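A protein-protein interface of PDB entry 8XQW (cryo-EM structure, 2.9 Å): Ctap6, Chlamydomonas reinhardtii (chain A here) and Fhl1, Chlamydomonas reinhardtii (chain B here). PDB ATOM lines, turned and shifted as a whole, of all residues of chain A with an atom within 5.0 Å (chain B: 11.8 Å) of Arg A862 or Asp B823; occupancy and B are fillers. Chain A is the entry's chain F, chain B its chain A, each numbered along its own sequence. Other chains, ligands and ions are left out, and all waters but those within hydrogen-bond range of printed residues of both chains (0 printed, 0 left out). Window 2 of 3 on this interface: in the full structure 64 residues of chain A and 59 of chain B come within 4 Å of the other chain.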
ATOM      1  N   ALA A 825     -17.000  -7.076 -14.781  1.00  0.00           N
ATOM      2  CA  ALA A 825     -17.211  -6.246 -13.605  1.00  0.00           C
ATOM      3  C   ALA A 825     -16.762  -4.808 -13.800  1.00  0.00           C
ATOM      4  O   ALA A 825     -16.951  -3.993 -12.895  1.00  0.00           O
ATOM      5  CB  ALA A 825     -16.483  -6.839 -12.406  1.00  0.00           C
ATOM      6  N   THR A 860     -16.979  -3.628  -4.412  1.00  0.00           N
ATOM      7  CA  THR A 860     -16.931  -4.998  -3.939  1.00  0.00           C
ATOM      8  C   THR A 860     -15.521  -5.561  -4.074  1.00  0.00           C
ATOM      9  O   THR A 860     -14.551  -4.839  -4.289  1.00  0.00           O
ATOM     10  CB  THR A 860     -17.949  -5.841  -4.691  1.00  0.00           C
ATOM     11  OG1 THR A 860     -17.790  -5.634  -6.093  1.00  0.00           O
ATOM     12  CG2 THR A 860     -19.334  -5.421  -4.307  1.00  0.00           C
ATOM     13  N   TYR A 861     -15.399  -6.874  -3.903  1.00  0.00           N
ATOM     14  CA  TYR A 861     -14.099  -7.533  -3.964  1.00  0.00           C
ATOM     15  C   TYR A 861     -13.797  -8.020  -5.373  1.00  0.00           C
ATOM     16  O   TYR A 861     -12.673  -7.858  -5.875  1.00  0.00           O
ATOM     17  CB  TYR A 861     -14.088  -8.686  -2.968  1.00  0.00           C
ATOM     18  CG  TYR A 861     -12.976  -9.679  -3.113  1.00  0.00           C
ATOM     19  CD1 TYR A 861     -11.685  -9.347  -2.785  1.00  0.00           C
ATOM     20  CD2 TYR A 861     -13.229 -10.962  -3.538  1.00  0.00           C
ATOM     21  CE1 TYR A 861     -10.681 -10.247  -2.903  1.00  0.00           C
ATOM     22  CE2 TYR A 861     -12.232 -11.870  -3.658  1.00  0.00           C
ATOM     23  CZ  TYR A 861     -10.957 -11.509  -3.339  1.00  0.00           C
ATOM     24  OH  TYR A 861      -9.943 -12.422  -3.452  1.00  0.00           O
ATOM     25  N   ARG A 862     -14.798  -8.622  -6.010  1.00  0.00           N
ATOM     26  CA  ARG A 862     -14.730  -8.957  -7.424  1.00  0.00           C
ATOM     27  C   ARG A 862     -14.205  -7.791  -8.244  1.00  0.00           C
ATOM     28  O   ARG A 862     -13.267  -7.935  -9.038  1.00  0.00           O
ATOM     29  CB  ARG A 862     -16.123  -9.357  -7.892  1.00  0.00           C
ATOM     30  CG  ARG A 862     -16.179 -10.003  -9.232  1.00  0.00           C
ATOM     31  CD  ARG A 862     -17.608 -10.314  -9.575  1.00  0.00           C
ATOM     32  NE  ARG A 862     -17.706 -11.220 -10.707  1.00  0.00           N
ATOM     33  CZ  ARG A 862     -17.945 -12.518 -10.594  1.00  0.00           C
ATOM     34  NH1 ARG A 862     -18.110 -13.057  -9.396  1.00  0.00           N
ATOM     35  NH2 ARG A 862     -18.018 -13.280 -11.675  1.00  0.00           N
ATOM     36  N   TYR A 863     -14.794  -6.617  -8.044  1.00  0.00           N
ATOM     37  CA  TYR A 863     -14.391  -5.452  -8.810  1.00  0.00           C
ATOM     38  C   TYR A 863     -12.937  -5.098  -8.575  1.00  0.00           C
ATOM     39  O   TYR A 863     -12.250  -4.664  -9.497  1.00  0.00           O
ATOM     40  CB  TYR A 863     -15.268  -4.270  -8.464  1.00  0.00           C
ATOM     41  CG  TYR A 863     -14.850  -3.041  -9.197  1.00  0.00           C
ATOM     42  CD1 TYR A 863     -15.153  -2.878 -10.528  1.00  0.00           C
ATOM     43  CD2 TYR A 863     -14.143  -2.045  -8.569  1.00  0.00           C
ATOM     44  CE1 TYR A 863     -14.770  -1.765 -11.204  1.00  0.00           C
ATOM     45  CE2 TYR A 863     -13.763  -0.927  -9.240  1.00  0.00           C
ATOM     46  CZ  TYR A 863     -14.074  -0.795 -10.554  1.00  0.00           C
ATOM     47  OH  TYR A 863     -13.694   0.327 -11.236  1.00  0.00           O
ATOM     48  N   LEU A 864     -12.447  -5.257  -7.352  1.00  0.00           N
ATOM     49  CA  LEU A 864     -11.057  -4.908  -7.092  1.00  0.00           C
ATOM     50  C   LEU A 864     -10.106  -5.868  -7.795  1.00  0.00           C
ATOM     51  O   LEU A 864      -9.084  -5.444  -8.350  1.00  0.00           O
ATOM     52  CB  LEU A 864     -10.794  -4.881  -5.594  1.00  0.00           C
ATOM     53  CG  LEU A 864     -11.288  -3.635  -4.864  1.00  0.00           C
ATOM     54  CD1 LEU A 864     -10.727  -3.596  -3.481  1.00  0.00           C
ATOM     55  CD2 LEU A 864     -10.882  -2.406  -5.604  1.00  0.00           C
ATOM     56  N   ARG A 865     -10.432  -7.159  -7.813  1.00  0.00           N
ATOM     57  CA  ARG A 865      -9.605  -8.088  -8.579  1.00  0.00           C
ATOM     58  C   ARG A 865      -9.560  -7.699 -10.057  1.00  0.00           C
ATOM     59  O   ARG A 865      -8.483  -7.646 -10.678  1.00  0.00           O
ATOM     60  CB  ARG A 865     -10.128  -9.509  -8.419  1.00  0.00           C
ATOM     61  CG  ARG A 865     -10.166  -9.993  -7.001  1.00  0.00           C
ATOM     62  CD  ARG A 865      -8.812  -9.892  -6.357  1.00  0.00           C
ATOM     63  NE  ARG A 865      -7.855 -10.828  -6.928  1.00  0.00           N
ATOM     64  CZ  ARG A 865      -7.841 -12.131  -6.679  1.00  0.00           C
ATOM     65  NH1 ARG A 865      -8.737 -12.663  -5.868  1.00  0.00           N
ATOM     66  NH2 ARG A 865      -6.931 -12.905  -7.243  1.00  0.00           N
ATOM     67  N   GLU A 866     -10.723  -7.414 -10.641  1.00  0.00           N
ATOM     68  CA  GLU A 866     -10.729  -7.066 -12.057  1.00  0.00           C
ATOM     69  C   GLU A 866     -10.001  -5.758 -12.313  1.00  0.00           C
ATOM     70  O   GLU A 866      -9.361  -5.602 -13.356  1.00  0.00           O
ATOM     71  CB  GLU A 866     -12.151  -6.990 -12.584  1.00  0.00           C
ATOM     72  CG  GLU A 866     -13.042  -8.049 -12.022  1.00  0.00           C
ATOM     73  CD  GLU A 866     -13.501  -9.047 -13.042  1.00  0.00           C
ATOM     74  OE1 GLU A 866     -14.692  -9.411 -13.024  1.00  0.00           O
ATOM     75  OE2 GLU A 866     -12.665  -9.490 -13.850  1.00  0.00           O
ATOM     76  N   TRP A1018     -23.103 -12.084 -17.574  1.00  0.00           N
ATOM     77  CA  TRP A1018     -23.234 -11.038 -16.568  1.00  0.00           C
ATOM     78  C   TRP A1018     -23.616  -9.696 -17.172  1.00  0.00           C
ATOM     79  O   TRP A1018     -23.169  -8.653 -16.689  1.00  0.00           O
ATOM     80  CB  TRP A1018     -21.934 -10.896 -15.785  1.00  0.00           C
ATOM     81  CG  TRP A1018     -21.536 -12.139 -15.112  1.00  0.00           C
ATOM     82  CD1 TRP A1018     -20.657 -13.067 -15.564  1.00  0.00           C
ATOM     83  CD2 TRP A1018     -22.009 -12.609 -13.853  1.00  0.00           C
ATOM     84  NE1 TRP A1018     -20.547 -14.091 -14.664  1.00  0.00           N
ATOM     85  CE2 TRP A1018     -21.371 -13.832 -13.601  1.00  0.00           C
ATOM     86  CE3 TRP A1018     -22.912 -12.113 -12.912  1.00  0.00           C
ATOM     87  CZ2 TRP A1018     -21.606 -14.568 -12.450  1.00  0.00           C
ATOM     88  CZ3 TRP A1018     -23.143 -12.842 -11.775  1.00  0.00           C
ATOM     89  CH2 TRP A1018     -22.493 -14.056 -11.550  1.00  0.00           C
ATOM     90  N   LEU A1024     -21.955  -5.422  -9.206  1.00  0.00           N
ATOM     91  CA  LEU A1024     -21.293  -6.712  -9.105  1.00  0.00           C
ATOM     92  C   LEU A1024     -20.216  -6.685  -8.027  1.00  0.00           C
ATOM     93  O   LEU A1024     -19.470  -5.715  -7.909  1.00  0.00           O
ATOM     94  CB  LEU A1024     -20.682  -7.095 -10.450  1.00  0.00           C
ATOM     95  CG  LEU A1024     -21.592  -7.852 -11.408  1.00  0.00           C
ATOM     96  CD1 LEU A1024     -21.220  -7.501 -12.817  1.00  0.00           C
ATOM     97  CD2 LEU A1024     -21.469  -9.339 -11.193  1.00  0.00           C
ATOM     98  OXT LEU A1024     -20.060  -7.631  -7.255  1.00  0.00           O
ATOM     99  N   GLU B 716     -29.114   0.202  -6.819  1.00  0.00           N
ATOM    100  CA  GLU B 716     -28.946  -1.039  -6.084  1.00  0.00           C
ATOM    101  C   GLU B 716     -27.790  -0.949  -5.110  1.00  0.00           C
ATOM    102  O   GLU B 716     -27.686  -1.782  -4.208  1.00  0.00           O
ATOM    103  CB  GLU B 716     -28.735  -2.207  -7.038  1.00  0.00           C
ATOM    104  CG  GLU B 716     -28.973  -3.552  -6.396  1.00  0.00           C
ATOM    105  CD  GLU B 716     -28.268  -4.676  -7.119  1.00  0.00           C
ATOM    106  OE1 GLU B 716     -28.565  -4.902  -8.309  1.00  0.00           O
ATOM    107  OE2 GLU B 716     -27.408  -5.329  -6.498  1.00  0.00           O
ATOM    108  N   ARG B 720     -27.820  -2.009  -0.733  1.00  0.00           N
ATOM    109  CA  ARG B 720     -26.789  -2.667   0.056  1.00  0.00           C
ATOM    110  C   ARG B 720     -26.272  -1.754   1.156  1.00  0.00           C
ATOM    111  O   ARG B 720     -25.981  -2.215   2.265  1.00  0.00           O
ATOM    112  CB  ARG B 720     -25.656  -3.124  -0.851  1.00  0.00           C
ATOM    113  CG  ARG B 720     -26.080  -4.195  -1.822  1.00  0.00           C
ATOM    114  CD  ARG B 720     -24.902  -4.755  -2.573  1.00  0.00           C
ATOM    115  NE  ARG B 720     -25.289  -5.872  -3.425  1.00  0.00           N
ATOM    116  CZ  ARG B 720     -24.427  -6.647  -4.072  1.00  0.00           C
ATOM    117  NH1 ARG B 720     -23.128  -6.426  -3.967  1.00  0.00           N
ATOM    118  NH2 ARG B 720     -24.865  -7.643  -4.826  1.00  0.00           N
ATOM    119  N   ILE B 724     -26.367  -2.779   5.163  1.00  0.00           N
ATOM    120  CA  ILE B 724     -25.265  -2.845   6.117  1.00  0.00           C
ATOM    121  C   ILE B 724     -25.479  -1.860   7.257  1.00  0.00           C
ATOM    122  O   ILE B 724     -25.121  -2.148   8.405  1.00  0.00           O
ATOM    123  CB  ILE B 724     -23.898  -2.636   5.440  1.00  0.00           C
ATOM    124  CG1 ILE B 724     -23.636  -1.168   5.155  1.00  0.00           C
ATOM    125  CG2 ILE B 724     -23.780  -3.472   4.189  1.00  0.00           C
ATOM    126  CD1 ILE B 724     -22.377  -0.932   4.400  1.00  0.00           C
ATOM    127  N   GLY B 812     -21.747  -5.396   9.865  1.00  0.00           N
ATOM    128  CA  GLY B 812     -21.898  -5.121   8.445  1.00  0.00           C
ATOM    129  C   GLY B 812     -21.241  -6.176   7.577  1.00  0.00           C
ATOM    130  O   GLY B 812     -21.871  -6.752   6.682  1.00  0.00           O
ATOM    131  N   ARG B 813     -19.958  -6.433   7.825  1.00  0.00           N
ATOM    132  CA  ARG B 813     -19.238  -7.442   7.064  1.00  0.00           C
ATOM    133  C   ARG B 813     -19.895  -8.802   7.185  1.00  0.00           C
ATOM    134  O   ARG B 813     -19.906  -9.569   6.221  1.00  0.00           O
ATOM    135  CB  ARG B 813     -17.793  -7.507   7.535  1.00  0.00           C
ATOM    136  CG  ARG B 813     -16.945  -8.493   6.782  1.00  0.00           C
ATOM    137  CD  ARG B 813     -16.863  -8.155   5.314  1.00  0.00           C
ATOM    138  NE  ARG B 813     -16.066  -6.964   5.062  1.00  0.00           N
ATOM    139  CZ  ARG B 813     -14.807  -6.985   4.656  1.00  0.00           C
ATOM    140  NH1 ARG B 813     -14.203  -8.140   4.459  1.00  0.00           N
ATOM    141  NH2 ARG B 813     -14.158  -5.857   4.444  1.00  0.00           N
ATOM    142  N   ALA B 814     -20.462  -9.114   8.345  1.00  0.00           N
ATOM    143  CA  ALA B 814     -21.105 -10.409   8.511  1.00  0.00           C
ATOM    144  C   ALA B 814     -22.393 -10.489   7.715  1.00  0.00           C
ATOM    145  O   ALA B 814     -22.698 -11.531   7.134  1.00  0.00           O
ATOM    146  CB  ALA B 814     -21.377 -10.674   9.982  1.00  0.00           C
ATOM    147  N   ALA B 815     -23.156  -9.399   7.668  1.00  0.00           N
ATOM    148  CA  ALA B 815     -24.351  -9.365   6.832  1.00  0.00           C
ATOM    149  C   ALA B 815     -23.996  -9.602   5.373  1.00  0.00           C
ATOM    150  O   ALA B 815     -24.629 -10.412   4.685  1.00  0.00           O
ATOM    151  CB  ALA B 815     -25.063  -8.026   6.995  1.00  0.00           C
ATOM    152  N   GLU B 816     -22.964  -8.909   4.892  1.00  0.00           N
ATOM    153  CA  GLU B 816     -22.539  -9.086   3.508  1.00  0.00           C
ATOM    154  C   GLU B 816     -22.108 -10.518   3.239  1.00  0.00           C
ATOM    155  O   GLU B 816     -22.634 -11.174   2.337  1.00  0.00           O
ATOM    156  CB  GLU B 816     -21.414  -8.120   3.183  1.00  0.00           C
ATOM    157  CG  GLU B 816     -21.814  -6.688   3.377  1.00  0.00           C
ATOM    158  CD  GLU B 816     -20.943  -5.737   2.606  1.00  0.00           C
ATOM    159  OE1 GLU B 816     -21.411  -5.204   1.579  1.00  0.00           O
ATOM    160  OE2 GLU B 816     -19.787  -5.522   3.023  1.00  0.00           O
ATOM    161  N   VAL B 817     -21.152 -11.027   4.017  1.00  0.00           N
ATOM    162  CA  VAL B 817     -20.656 -12.377   3.787  1.00  0.00           C
ATOM    163  C   VAL B 817     -21.765 -13.409   3.939  1.00  0.00           C
ATOM    164  O   VAL B 817     -21.706 -14.484   3.337  1.00  0.00           O
ATOM    165  CB  VAL B 817     -19.484 -12.665   4.735  1.00  0.00           C
ATOM    166  CG1 VAL B 817     -19.067 -14.104   4.650  1.00  0.00           C
ATOM    167  CG2 VAL B 817     -18.323 -11.781   4.395  1.00  0.00           C
ATOM    168  N   ALA B 818     -22.804 -13.107   4.713  1.00  0.00           N
ATOM    169  CA  ALA B 818     -23.877 -14.076   4.869  1.00  0.00           C
ATOM    170  C   ALA B 818     -24.814 -14.061   3.674  1.00  0.00           C
ATOM    171  O   ALA B 818     -25.326 -15.108   3.267  1.00  0.00           O
ATOM    172  CB  ALA B 818     -24.647 -13.794   6.154  1.00  0.00           C
ATOM    173  N   LEU B 819     -25.053 -12.886   3.094  1.00  0.00           N
ATOM    174  CA  LEU B 819     -26.016 -12.812   2.001  1.00  0.00           C
ATOM    175  C   LEU B 819     -25.376 -13.053   0.638  1.00  0.00           C
ATOM    176  O   LEU B 819     -26.007 -13.637  -0.247  1.00  0.00           O
ATOM    177  CB  LEU B 819     -26.728 -11.464   2.024  1.00  0.00           C
ATOM    178  CG  LEU B 819     -28.070 -11.431   2.747  1.00  0.00           C
ATOM    179  CD1 LEU B 819     -28.104 -12.396   3.909  1.00  0.00           C
ATOM    180  CD2 LEU B 819     -28.340 -10.031   3.233  1.00  0.00           C
ATOM    181  N   PHE B 820     -24.136 -12.620   0.443  1.00  0.00           N
ATOM    182  CA  PHE B 820     -23.524 -12.678  -0.872  1.00  0.00           C
ATOM    183  C   PHE B 820     -22.309 -13.586  -0.958  1.00  0.00           C
ATOM    184  O   PHE B 820     -22.085 -14.182  -2.015  1.00  0.00           O
ATOM    185  CB  PHE B 820     -23.112 -11.273  -1.331  1.00  0.00           C
ATOM    186  CG  PHE B 820     -24.190 -10.246  -1.185  1.00  0.00           C
ATOM    187  CD1 PHE B 820     -25.504 -10.559  -1.457  1.00  0.00           C
ATOM    188  CD2 PHE B 820     -23.887  -8.964  -0.784  1.00  0.00           C
ATOM    189  CE1 PHE B 820     -26.488  -9.617  -1.323  1.00  0.00           C
ATOM    190  CE2 PHE B 820     -24.871  -8.021  -0.651  1.00  0.00           C
ATOM    191  CZ  PHE B 820     -26.170  -8.350  -0.917  1.00  0.00           C
ATOM    192  N   GLY B 821     -21.529 -13.715   0.098  1.00  0.00           N
ATOM    193  CA  GLY B 821     -20.270 -14.418   0.015  1.00  0.00           C
ATOM    194  C   GLY B 821     -19.121 -13.450  -0.121  1.00  0.00           C
ATOM    195  O   GLY B 821     -19.301 -12.234  -0.200  1.00  0.00           O
ATOM    196  N   LYS B 822     -17.910 -14.009  -0.161  1.00  0.00           N
ATOM    197  CA  LYS B 822     -16.718 -13.166  -0.188  1.00  0.00           C
ATOM    198  C   LYS B 822     -16.747 -12.169  -1.336  1.00  0.00           C
ATOM    199  O   LYS B 822     -16.155 -11.094  -1.225  1.00  0.00           O
ATOM    200  CB  LYS B 822     -15.459 -14.016  -0.280  1.00  0.00           C
ATOM    201  CG  LYS B 822     -14.202 -13.260   0.103  1.00  0.00           C
ATOM    202  CD  LYS B 822     -12.953 -14.016  -0.301  1.00  0.00           C
ATOM    203  CE  LYS B 822     -11.716 -13.451   0.370  1.00  0.00           C
ATOM    204  NZ  LYS B 822     -11.951 -12.097   0.922  1.00  0.00           N
ATOM    205  N   ASP B 823     -17.430 -12.493  -2.434  1.00  0.00           N
ATOM    206  CA  ASP B 823     -17.533 -11.549  -3.538  1.00  0.00           C
ATOM    207  C   ASP B 823     -18.290 -10.292  -3.155  1.00  0.00           C
ATOM    208  O   ASP B 823     -18.121  -9.260  -3.812  1.00  0.00           O
ATOM    209  CB  ASP B 823     -18.222 -12.209  -4.721  1.00  0.00           C
ATOM    210  CG  ASP B 823     -17.729 -13.604  -4.958  1.00  0.00           C
ATOM    211  OD1 ASP B 823     -17.545 -14.335  -3.964  1.00  0.00           O
ATOM    212  OD2 ASP B 823     -17.519 -13.971  -6.131  1.00  0.00           O
ATOM    213  N   GLY B 824     -19.118 -10.351  -2.120  1.00  0.00           N
ATOM    214  CA  GLY B 824     -19.887  -9.217  -1.669  1.00  0.00           C
ATOM    215  C   GLY B 824     -19.211  -8.360  -0.632  1.00  0.00           C
ATOM    216  O   GLY B 824     -19.748  -7.311  -0.275  1.00  0.00           O
ATOM    217  N   ALA B 825     -18.055  -8.771  -0.132  1.00  0.00           N
ATOM    218  CA  ALA B 825     -17.327  -7.960   0.829  1.00  0.00           C
ATOM    219  C   ALA B 825     -16.852  -6.674   0.179  1.00  0.00           C
ATOM    220  O   ALA B 825     -16.115  -6.699  -0.801  1.00  0.00           O
ATOM    221  CB  ALA B 825     -16.139  -8.739   1.370  1.00  0.00           C
ATOM    222  N   SER B 826     -17.257  -5.544   0.738  1.00  0.00           N
ATOM    223  CA  SER B 826     -17.039  -4.259   0.100  1.00  0.00           C
ATOM    224  C   SER B 826     -16.011  -3.456   0.875  1.00  0.00           C
ATOM    225  O   SER B 826     -15.495  -3.889   1.902  1.00  0.00           O
ATOM    226  CB  SER B 826     -18.345  -3.471   0.003  1.00  0.00           C
ATOM    227  OG  SER B 826     -18.385  -2.477   1.000  1.00  0.00           O
ATOM    228  N   LEU B 827     -15.714  -2.264   0.371  1.00  0.00           N
ATOM    229  CA  LEU B 827     -14.903  -1.305   1.105  1.00  0.00           C
ATOM    230  C   LEU B 827     -15.725  -0.471   2.066  1.00  0.00           C
ATOM    231  O   LEU B 827     -15.152   0.315   2.823  1.00  0.00           O
ATOM    232  CB  LEU B 827     -14.179  -0.357   0.151  1.00  0.00           C
ATOM    233  CG  LEU B 827     -13.066  -0.842  -0.763  1.00  0.00           C
ATOM    234  CD1 LEU B 827     -12.054   0.246  -0.911  1.00  0.00           C
ATOM    235  CD2 LEU B 827     -12.424  -2.070  -0.206  1.00  0.00           C
ATOM    236  N   ALA B 828     -17.045  -0.586   2.031  1.00  0.00           N
ATOM    237  CA  ALA B 828     -17.862   0.161   2.970  1.00  0.00           C
ATOM    238  C   ALA B 828     -17.761  -0.396   4.374  1.00  0.00           C
ATOM    239  O   ALA B 828     -17.830   0.367   5.340  1.00  0.00           O
ATOM    240  CB  ALA B 828     -19.323   0.150   2.526  1.00  0.00           C
ATOM    241  N   THR B 829     -17.573  -1.704   4.497  1.00  0.00           N
ATOM    242  CA  THR B 829     -17.605  -2.396   5.774  1.00  0.00           C
ATOM    243  C   THR B 829     -16.215  -2.661   6.325  1.00  0.00           C
ATOM    244  O   THR B 829     -16.082  -3.280   7.377  1.00  0.00           O
ATOM    245  CB  THR B 829     -18.368  -3.703   5.620  1.00  0.00           C
ATOM    246  OG1 THR B 829     -17.865  -4.402   4.485  1.00  0.00           O
ATOM    247  CG2 THR B 829     -19.807  -3.412   5.383  1.00  0.00           C
ATOM    248  N   TRP B 900     -15.968 -13.049  15.613  1.00  0.00           N
ATOM    249  CA  TRP B 900     -16.483 -13.167  14.255  1.00  0.00           C
ATOM    250  C   TRP B 900     -17.587 -14.211  14.176  1.00  0.00           C
ATOM    251  O   TRP B 900     -18.626 -13.978  13.549  1.00  0.00           O
ATOM    252  CB  TRP B 900     -15.351 -13.501  13.283  1.00  0.00           C
ATOM    253  CG  TRP B 900     -15.828 -13.939  11.950  1.00  0.00           C
ATOM    254  CD1 TRP B 900     -15.783 -15.193  11.440  1.00  0.00           C
ATOM    255  CD2 TRP B 900     -16.429 -13.122  10.951  1.00  0.00           C
ATOM    256  NE1 TRP B 900     -16.325 -15.212  10.186  1.00  0.00           N
ATOM    257  CE2 TRP B 900     -16.732 -13.947   9.866  1.00  0.00           C
ATOM    258  CE3 TRP B 900     -16.746 -11.770  10.875  1.00  0.00           C
ATOM    259  CZ2 TRP B 900     -17.326 -13.468   8.721  1.00  0.00           C
ATOM    260  CZ3 TRP B 900     -17.330 -11.300   9.743  1.00  0.00           C
ATOM    261  CH2 TRP B 900     -17.621 -12.141   8.682  1.00  0.00           C
ATOM    262  N   LEU B 951     -28.252 -18.195   3.081  1.00  0.00           N
ATOM    263  CA  LEU B 951     -27.026 -18.045   3.852  1.00  0.00           C
ATOM    264  C   LEU B 951     -25.780 -18.459   3.079  1.00  0.00           C
ATOM    265  O   LEU B 951     -24.839 -18.999   3.671  1.00  0.00           O
ATOM    266  CB  LEU B 951     -27.126 -18.826   5.161  1.00  0.00           C
ATOM    267  CG  LEU B 951     -28.224 -18.322   6.091  1.00  0.00           C
ATOM    268  CD1 LEU B 951     -28.097 -18.969   7.451  1.00  0.00           C
ATOM    269  CD2 LEU B 951     -28.167 -16.809   6.194  1.00  0.00           C
ATOM    270  N   ASP B 952     -25.771 -18.258   1.760  1.00  0.00           N
ATOM    271  CA  ASP B 952     -24.537 -18.289   0.982  1.00  0.00           C
ATOM    272  C   ASP B 952     -23.922 -19.683   0.898  1.00  0.00           C
ATOM    273  O   ASP B 952     -22.978 -19.908   0.134  1.00  0.00           O
ATOM    274  CB  ASP B 952     -23.544 -17.284   1.582  1.00  0.00           C
ATOM    275  CG  ASP B 952     -22.136 -17.445   1.051  1.00  0.00           C
ATOM    276  OD1 ASP B 952     -21.886 -17.076  -0.114  1.00  0.00           O
ATOM    277  OD2 ASP B 952     -21.278 -17.945   1.806  1.00  0.00           O
ATOM    278  N   GLY B 953     -24.467 -20.641   1.630  1.00  0.00           N
ATOM    279  CA  GLY B 953     -23.892 -21.982   1.594  1.00  0.00           C
ATOM    280  C   GLY B 953     -22.573 -22.133   2.315  1.00  0.00           C
ATOM    281  O   GLY B 953     -22.402 -23.064   3.106  1.00  0.00           O
ATOM    282  N   ALA B 954     -21.618 -21.238   2.053  1.00  0.00           N
ATOM    283  CA  ALA B 954     -20.349 -21.293   2.769  1.00  0.00           C
ATOM    284  C   ALA B 954     -20.507 -20.802   4.201  1.00  0.00           C
ATOM    285  O   ALA B 954     -20.117 -21.497   5.148  1.00  0.00           O
ATOM    286  CB  ALA B 954     -19.288 -20.475   2.035  1.00  0.00           C
ATOM    287  N   ALA B 955     -21.080 -19.613   4.383  1.00  0.00           N
ATOM    288  CA  ALA B 955     -21.367 -19.119   5.721  1.00  0.00           C
ATOM    289  C   ALA B 955     -22.488 -19.887   6.399  1.00  0.00           C
ATOM    290  O   ALA B 955     -22.736 -19.667   7.587  1.00  0.00           O
ATOM    291  CB  ALA B 955     -21.726 -17.635   5.673  1.00  0.00           C
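Of chain B, only Asp B823 comes within 4 Å of Arg A862.
Of chain A, only Thr A860, Tyr A861 and Arg A862 come within 4 Å of Asp B823.
No residue of chain B comes within 4 Å of Ala A825.
Thr A860 touches just these residues of chain B: Arg B720 (3.9 Å), Asp B823 (3.5 Å) and Ala B825 (3.5 Å).
Of chain B, only Lys B822, Asp B823 and Ala B825 come within 4 Å of Tyr A861.
No residue of chain B comes within 4 Å of Glu A866.
No residue of chain B comes within 4 Å of Leu A1024.
Printed residues of chain A within 4 Å of Leu B827: Leu A864 (3.99 Å).
Printed residues of chain A within 4 Å of Lys B822: Tyr A861.
Printed residues of chain A within 4 Å of Ala B825: Thr A860 (3.5 Å) and Tyr A861 (3.2 Å).
Of the printed residues of chain A, Arg B720 touches Thr A860 (3.9 Å).
Arg A865 touches none of the printed residues of chain B.
The nearest residue of chain A that does not touch Asp B823 is Leu A1024 (4.3 Å).
OE2 of Glu B716 lies within salt-bridge range of NE of Arg B720 (3.8 Å).
The chain-end carboxylate (O) of Leu A1024 sits at hydrogen-bond distance from the side-chain hydroxyl (OG1) of Thr A860.
OH of Tyr A861 sits at hydrogen-bond distance from NH1 of Arg A865 (2.7 Å).
Hydrophobic or aromatic side chains of chain A that line the printed part of chain B: Tyr A861 and Leu A864.
Among the printed residues, Asp or Glu carboxylates within 4 Å of a Lys or Arg side-chain nitrogen of the other chain: Arg A862 with Asp B823.
Among the printed residues, merely in contact across the chains: Thr A860 with Arg B720 (3.9 Å), Thr A860 with Asp B823 (3.5 Å), Thr A860 with Ala B825 (3.5 Å), Tyr A861 with Lys B822 (3.6 Å), Tyr A861 with Asp B823 (3.6 Å) and Leu A864 with Leu B827 (3.99 Å).
The side-chain carboxylate (OD2) of Asp B823 lies within salt-bridge range of the guanidinium group (NH1) of Arg A862 (3.4 Å).
O of Ala B825 sits at hydrogen-bond distance from N of Tyr A861, at 3.2 Å.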
